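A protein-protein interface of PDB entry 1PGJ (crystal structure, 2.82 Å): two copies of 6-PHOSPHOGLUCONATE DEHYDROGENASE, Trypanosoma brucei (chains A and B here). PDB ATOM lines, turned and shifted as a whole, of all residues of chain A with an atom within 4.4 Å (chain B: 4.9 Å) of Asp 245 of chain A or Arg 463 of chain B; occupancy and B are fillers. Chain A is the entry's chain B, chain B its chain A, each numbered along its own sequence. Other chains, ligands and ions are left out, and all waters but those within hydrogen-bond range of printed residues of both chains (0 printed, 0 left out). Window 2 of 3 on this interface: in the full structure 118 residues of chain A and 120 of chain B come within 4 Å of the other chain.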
ATOM      1  N   LYS A 244      20.464   3.589  -8.196  1.00  0.00           N
ATOM      2  CA  LYS A 244      21.803   3.814  -7.659  1.00  0.00           C
ATOM      3  C   LYS A 244      22.201   5.272  -7.690  1.00  0.00           C
ATOM      4  O   LYS A 244      21.828   6.029  -8.587  1.00  0.00           O
ATOM      5  CB  LYS A 244      22.866   3.000  -8.415  1.00  0.00           C
ATOM      6  CG  LYS A 244      22.996   1.570  -7.958  1.00  0.00           C
ATOM      7  CD  LYS A 244      23.775   0.738  -8.956  1.00  0.00           C
ATOM      8  CE  LYS A 244      23.692  -0.765  -8.618  1.00  0.00           C
ATOM      9  NZ  LYS A 244      22.276  -1.336  -8.618  1.00  0.00           N
ATOM     10  N   ASP A 245      22.975   5.651  -6.687  1.00  0.00           N
ATOM     11  CA  ASP A 245      23.468   7.004  -6.557  1.00  0.00           C
ATOM     12  C   ASP A 245      24.700   7.218  -7.442  1.00  0.00           C
ATOM     13  O   ASP A 245      25.281   6.259  -7.957  1.00  0.00           O
ATOM     14  CB  ASP A 245      23.820   7.280  -5.104  1.00  0.00           C
ATOM     15  CG  ASP A 245      23.809   8.759  -4.770  1.00  0.00           C
ATOM     16  OD1 ASP A 245      23.405   9.581  -5.626  1.00  0.00           O
ATOM     17  OD2 ASP A 245      24.188   9.095  -3.626  1.00  0.00           O
ATOM     18  N   LYS A 246      25.097   8.480  -7.596  1.00  0.00           N
ATOM     19  CA  LYS A 246      26.254   8.844  -8.402  1.00  0.00           C
ATOM     20  C   LYS A 246      27.505   8.112  -7.944  1.00  0.00           C
ATOM     21  O   LYS A 246      28.366   7.779  -8.752  1.00  0.00           O
ATOM     22  CB  LYS A 246      26.479  10.359  -8.393  1.00  0.00           C
ATOM     23  CG  LYS A 246      25.916  11.040  -9.639  1.00  0.00           C
ATOM     24  CD  LYS A 246      26.612  10.521 -10.927  1.00  0.00           C
ATOM     25  CE  LYS A 246      25.824  10.816 -12.233  1.00  0.00           C
ATOM     26  NZ  LYS A 246      25.036   9.634 -12.733  1.00  0.00           N
ATOM     27  N   ASP A 247      27.591   7.835  -6.646  1.00  0.00           N
ATOM     28  CA  ASP A 247      28.728   7.109  -6.080  1.00  0.00           C
ATOM     29  C   ASP A 247      28.628   5.604  -6.344  1.00  0.00           C
ATOM     30  O   ASP A 247      29.355   4.815  -5.727  1.00  0.00           O
ATOM     31  CB  ASP A 247      28.787   7.331  -4.575  1.00  0.00           C
ATOM     32  CG  ASP A 247      27.776   6.495  -3.830  1.00  0.00           C
ATOM     33  OD1 ASP A 247      26.581   6.493  -4.217  1.00  0.00           O
ATOM     34  OD2 ASP A 247      28.190   5.813  -2.871  1.00  0.00           O
ATOM     35  N   GLY A 248      27.665   5.216  -7.178  1.00  0.00           N
ATOM     36  CA  GLY A 248      27.464   3.819  -7.524  1.00  0.00           C
ATOM     37  C   GLY A 248      26.983   2.904  -6.411  1.00  0.00           C
ATOM     38  O   GLY A 248      27.272   1.701  -6.420  1.00  0.00           O
ATOM     39  N   SER A 249      26.276   3.458  -5.434  1.00  0.00           N
ATOM     40  CA  SER A 249      25.751   2.652  -4.345  1.00  0.00           C
ATOM     41  C   SER A 249      24.247   2.742  -4.448  1.00  0.00           C
ATOM     42  O   SER A 249      23.734   3.553  -5.205  1.00  0.00           O
ATOM     43  CB  SER A 249      26.177   3.248  -3.022  1.00  0.00           C
ATOM     44  OG  SER A 249      25.601   4.527  -2.880  1.00  0.00           O
ATOM     45  N   LEU A 251      20.584   3.894  -3.820  1.00  0.00           N
ATOM     46  CA  LEU A 251      19.981   5.156  -3.457  1.00  0.00           C
ATOM     47  C   LEU A 251      19.313   5.158  -2.102  1.00  0.00           C
ATOM     48  O   LEU A 251      19.467   6.111  -1.345  1.00  0.00           O
ATOM     49  CB  LEU A 251      18.974   5.571  -4.523  1.00  0.00           C
ATOM     50  CG  LEU A 251      18.653   7.061  -4.433  1.00  0.00           C
ATOM     51  CD1 LEU A 251      19.952   7.867  -4.540  1.00  0.00           C
ATOM     52  CD2 LEU A 251      17.673   7.450  -5.525  1.00  0.00           C
ATOM     53  N   HIS A 254      20.931   6.348   1.109  1.00  0.00           N
ATOM     54  CA  HIS A 254      21.192   7.765   1.330  1.00  0.00           C
ATOM     55  C   HIS A 254      19.897   8.515   1.568  1.00  0.00           C
ATOM     56  O   HIS A 254      19.912   9.741   1.699  1.00  0.00           O
ATOM     57  CB  HIS A 254      21.898   8.370   0.122  1.00  0.00           C
ATOM     58  CG  HIS A 254      23.137   7.629  -0.272  1.00  0.00           C
ATOM     59  ND1 HIS A 254      24.283   7.635   0.496  1.00  0.00           N
ATOM     60  CD2 HIS A 254      23.384   6.790  -1.306  1.00  0.00           C
ATOM     61  CE1 HIS A 254      25.177   6.829  -0.045  1.00  0.00           C
ATOM     62  NE2 HIS A 254      24.656   6.306  -1.139  1.00  0.00           N
ATOM     63  N   MET A 256      16.697   9.819   3.578  1.00  0.00           N
ATOM     64  CA  MET A 256      16.218  10.231   4.883  1.00  0.00           C
ATOM     65  C   MET A 256      14.867   9.566   5.125  1.00  0.00           C
ATOM     66  O   MET A 256      13.904   9.849   4.412  1.00  0.00           O
ATOM     67  CB  MET A 256      16.070  11.754   4.856  1.00  0.00           C
ATOM     68  CG  MET A 256      15.508  12.361   6.100  1.00  0.00           C
ATOM     69  SD  MET A 256      16.415  11.857   7.557  1.00  0.00           S
ATOM     70  CE  MET A 256      16.469  13.452   8.399  1.00  0.00           C
ATOM     71  N   TYR B 461      12.603  13.817  -2.156  1.00  0.00           N
ATOM     72  CA  TYR B 461      12.876  13.167  -0.883  1.00  0.00           C
ATOM     73  C   TYR B 461      14.073  13.804  -0.161  1.00  0.00           C
ATOM     74  O   TYR B 461      14.992  14.347  -0.788  1.00  0.00           O
ATOM     75  CB  TYR B 461      13.144  11.675  -1.107  1.00  0.00           C
ATOM     76  CG  TYR B 461      14.176  11.383  -2.176  1.00  0.00           C
ATOM     77  CD1 TYR B 461      15.546  11.445  -1.896  1.00  0.00           C
ATOM     78  CD2 TYR B 461      13.790  11.118  -3.488  1.00  0.00           C
ATOM     79  CE1 TYR B 461      16.522  11.262  -2.921  1.00  0.00           C
ATOM     80  CE2 TYR B 461      14.745  10.934  -4.515  1.00  0.00           C
ATOM     81  CZ  TYR B 461      16.113  11.012  -4.232  1.00  0.00           C
ATOM     82  OH  TYR B 461      17.045  10.877  -5.251  1.00  0.00           O
ATOM     83  N   GLU B 462      14.049  13.775   1.158  1.00  0.00           N
ATOM     84  CA  GLU B 462      15.150  14.324   1.899  1.00  0.00           C
ATOM     85  C   GLU B 462      16.248  13.284   1.846  1.00  0.00           C
ATOM     86  O   GLU B 462      15.995  12.085   1.679  1.00  0.00           O
ATOM     87  CB  GLU B 462      14.758  14.605   3.346  1.00  0.00           C
ATOM     88  CG  GLU B 462      13.548  15.498   3.486  1.00  0.00           C
ATOM     89  CD  GLU B 462      13.498  16.179   4.830  1.00  0.00           C
ATOM     90  OE1 GLU B 462      13.365  15.473   5.859  1.00  0.00           O
ATOM     91  OE2 GLU B 462      13.590  17.432   4.846  1.00  0.00           O
ATOM     92  N   ARG B 463      17.476  13.765   1.996  1.00  0.00           N
ATOM     93  CA  ARG B 463      18.670  12.938   1.968  1.00  0.00           C
ATOM     94  C   ARG B 463      19.304  13.080   3.314  1.00  0.00           C
ATOM     95  O   ARG B 463      19.190  14.123   3.944  1.00  0.00           O
ATOM     96  CB  ARG B 463      19.651  13.469   0.939  1.00  0.00           C
ATOM     97  CG  ARG B 463      19.673  12.730  -0.361  1.00  0.00           C
ATOM     98  CD  ARG B 463      21.100  12.319  -0.622  1.00  0.00           C
ATOM     99  NE  ARG B 463      21.359  12.074  -2.033  1.00  0.00           N
ATOM    100  CZ  ARG B 463      22.413  11.409  -2.499  1.00  0.00           C
ATOM    101  NH1 ARG B 463      23.319  10.902  -1.663  1.00  0.00           N
ATOM    102  NH2 ARG B 463      22.573  11.283  -3.811  1.00  0.00           N
ATOM    103  N   VAL B 464      20.029  12.053   3.717  1.00  0.00           N
ATOM    104  CA  VAL B 464      20.696  12.057   4.996  1.00  0.00           C
ATOM    105  C   VAL B 464      22.060  12.747   4.921  1.00  0.00           C
ATOM    106  O   VAL B 464      22.615  13.165   5.939  1.00  0.00           O
ATOM    107  CB  VAL B 464      20.882  10.613   5.525  1.00  0.00           C
ATOM    108  CG1 VAL B 464      19.533   9.927   5.665  1.00  0.00           C
ATOM    109  CG2 VAL B 464      21.798   9.824   4.622  1.00  0.00           C
ATOM    110  N   ASP B 465      22.581  12.896   3.709  1.00  0.00           N
ATOM    111  CA  ASP B 465      23.903  13.487   3.522  1.00  0.00           C
ATOM    112  C   ASP B 465      23.960  14.904   2.976  1.00  0.00           C
ATOM    113  O   ASP B 465      24.970  15.573   3.150  1.00  0.00           O
ATOM    114  CB  ASP B 465      24.763  12.562   2.664  1.00  0.00           C
ATOM    115  CG  ASP B 465      24.170  12.338   1.301  1.00  0.00           C
ATOM    116  OD1 ASP B 465      24.253  13.265   0.480  1.00  0.00           O
ATOM    117  OD2 ASP B 465      23.604  11.254   1.057  1.00  0.00           O
ATOM    118  N   LYS B 466      22.943  15.337   2.235  1.00  0.00           N
ATOM    119  CA  LYS B 466      22.953  16.705   1.713  1.00  0.00           C
ATOM    120  C   LYS B 466      22.067  17.559   2.607  1.00  0.00           C
ATOM    121  O   LYS B 466      22.205  17.544   3.829  1.00  0.00           O
ATOM    122  CB  LYS B 466      22.478  16.765   0.252  1.00  0.00           C
ATOM    123  CG  LYS B 466      23.398  16.049  -0.739  1.00  0.00           C
ATOM    124  CD  LYS B 466      23.128  16.446  -2.190  1.00  0.00           C
ATOM    125  CE  LYS B 466      23.782  15.469  -3.160  1.00  0.00           C
ATOM    126  NZ  LYS B 466      23.640  15.923  -4.569  1.00  0.00           N
ATOM    127  N   GLY B 468      18.021  19.852   1.977  1.00  0.00           N
ATOM    128  CA  GLY B 468      17.046  20.152   0.946  1.00  0.00           C
ATOM    129  C   GLY B 468      16.554  18.867   0.297  1.00  0.00           C
ATOM    130  O   GLY B 468      16.966  17.762   0.678  1.00  0.00           O
ATOM    131  N   GLU B 470      15.781  16.223  -3.003  1.00  0.00           N
ATOM    132  CA  GLU B 470      16.390  15.756  -4.230  1.00  0.00           C
ATOM    133  C   GLU B 470      15.350  14.979  -5.000  1.00  0.00           C
ATOM    134  O   GLU B 470      14.524  14.308  -4.411  1.00  0.00           O
ATOM    135  CB  GLU B 470      17.551  14.831  -3.942  1.00  0.00           C
ATOM    136  CG  GLU B 470      18.036  14.131  -5.188  1.00  0.00           C
ATOM    137  CD  GLU B 470      19.294  13.360  -4.966  1.00  0.00           C
ATOM    138  OE1 GLU B 470      20.116  13.809  -4.152  1.00  0.00           O
ATOM    139  OE2 GLU B 470      19.478  12.315  -5.618  1.00  0.00           O
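The guanidinium group (NH2) of Arg 463 of chain B lies within salt-bridge range of the side-chain carboxylate (OD1) of Asp 245 of chain A (2.6 Å).
The backbone carbonyl oxygen (O) of Glu 462 of chain B sits at hydrogen-bond distance from the backbone NH (N) of Met 256 of chain A (3.0 Å).
The backbone NH of Val 464 of chain B is in hydrogen-bond range of the backbone carbonyl oxygen of His 254 of chain A (3.1 Å).
OH of Tyr 461 of chain B is in hydrogen-bond range of OE2 of Glu 470 of chain B, at 2.8 Å.
NE2 of His 254 of chain A sits at hydrogen-bond distance from OG of Ser 249 of chain A (2.7 Å).
NH1 of Arg 463 of chain B is in salt-bridge range of OD2 of Asp 465 of chain B (2.8 Å).
The guanidinium group of Arg 463 of chain B lies within salt-bridge range of the side-chain carboxylate of Glu 470 of chain B (3.0 Å).
Among the printed residues, merely in contact across the chains: His 254 of chain A with Arg 463 of chain B, Met 256 of chain A with Val 464 of chain B, His 254 of chain A with Asp 465 of chain B, Leu 251 of chain A with Tyr 461 of chain B and Met 256 of chain A with Arg 463 of chain B.
Of the 9 printed residues of chain A, 4 touch a printed residue of chain B.
Of the 8 printed residues of chain B, 5 touch a printed residue of chain A.
Printed residues of chain B that touch a printed residue of chain A: Tyr 461, Glu 462, Arg 463, Val 464 and Asp 465.
Hydrophobic or aromatic side chains of chain B that line the printed part of chain A: Tyr 461 and Val 464.
Among the printed residues, 8 pairs touch across the chains.
No position is printed for both chains.
Asp 245 of chain A touches just one residue of chain B: Arg 463.
Of the printed residues of chain B, Leu 251 of chain A touches Tyr 461 (3.5 Å).
Of the printed residues of chain B, Met 256 of chain A touches Glu 462, Arg 463 and Val 464.
Printed residues of chain A within 4 Å of Tyr 461 of chain B: Leu 251 (3.5 Å).
Of the printed residues of chain A, Glu 462 of chain B touches Met 256.
Arg 463 of chain B touches three residues of chain A.
Lys 466 of chain B touches none of the printed residues of chain A.
The nearest residue of chain B that does not touch Asp 245 of chain A is Glu 470 of chain B (4.8 Å).
The nearest printed residue of chain A that does not touch Arg 463 of chain B is Leu 251 of chain A (4.4 Å).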
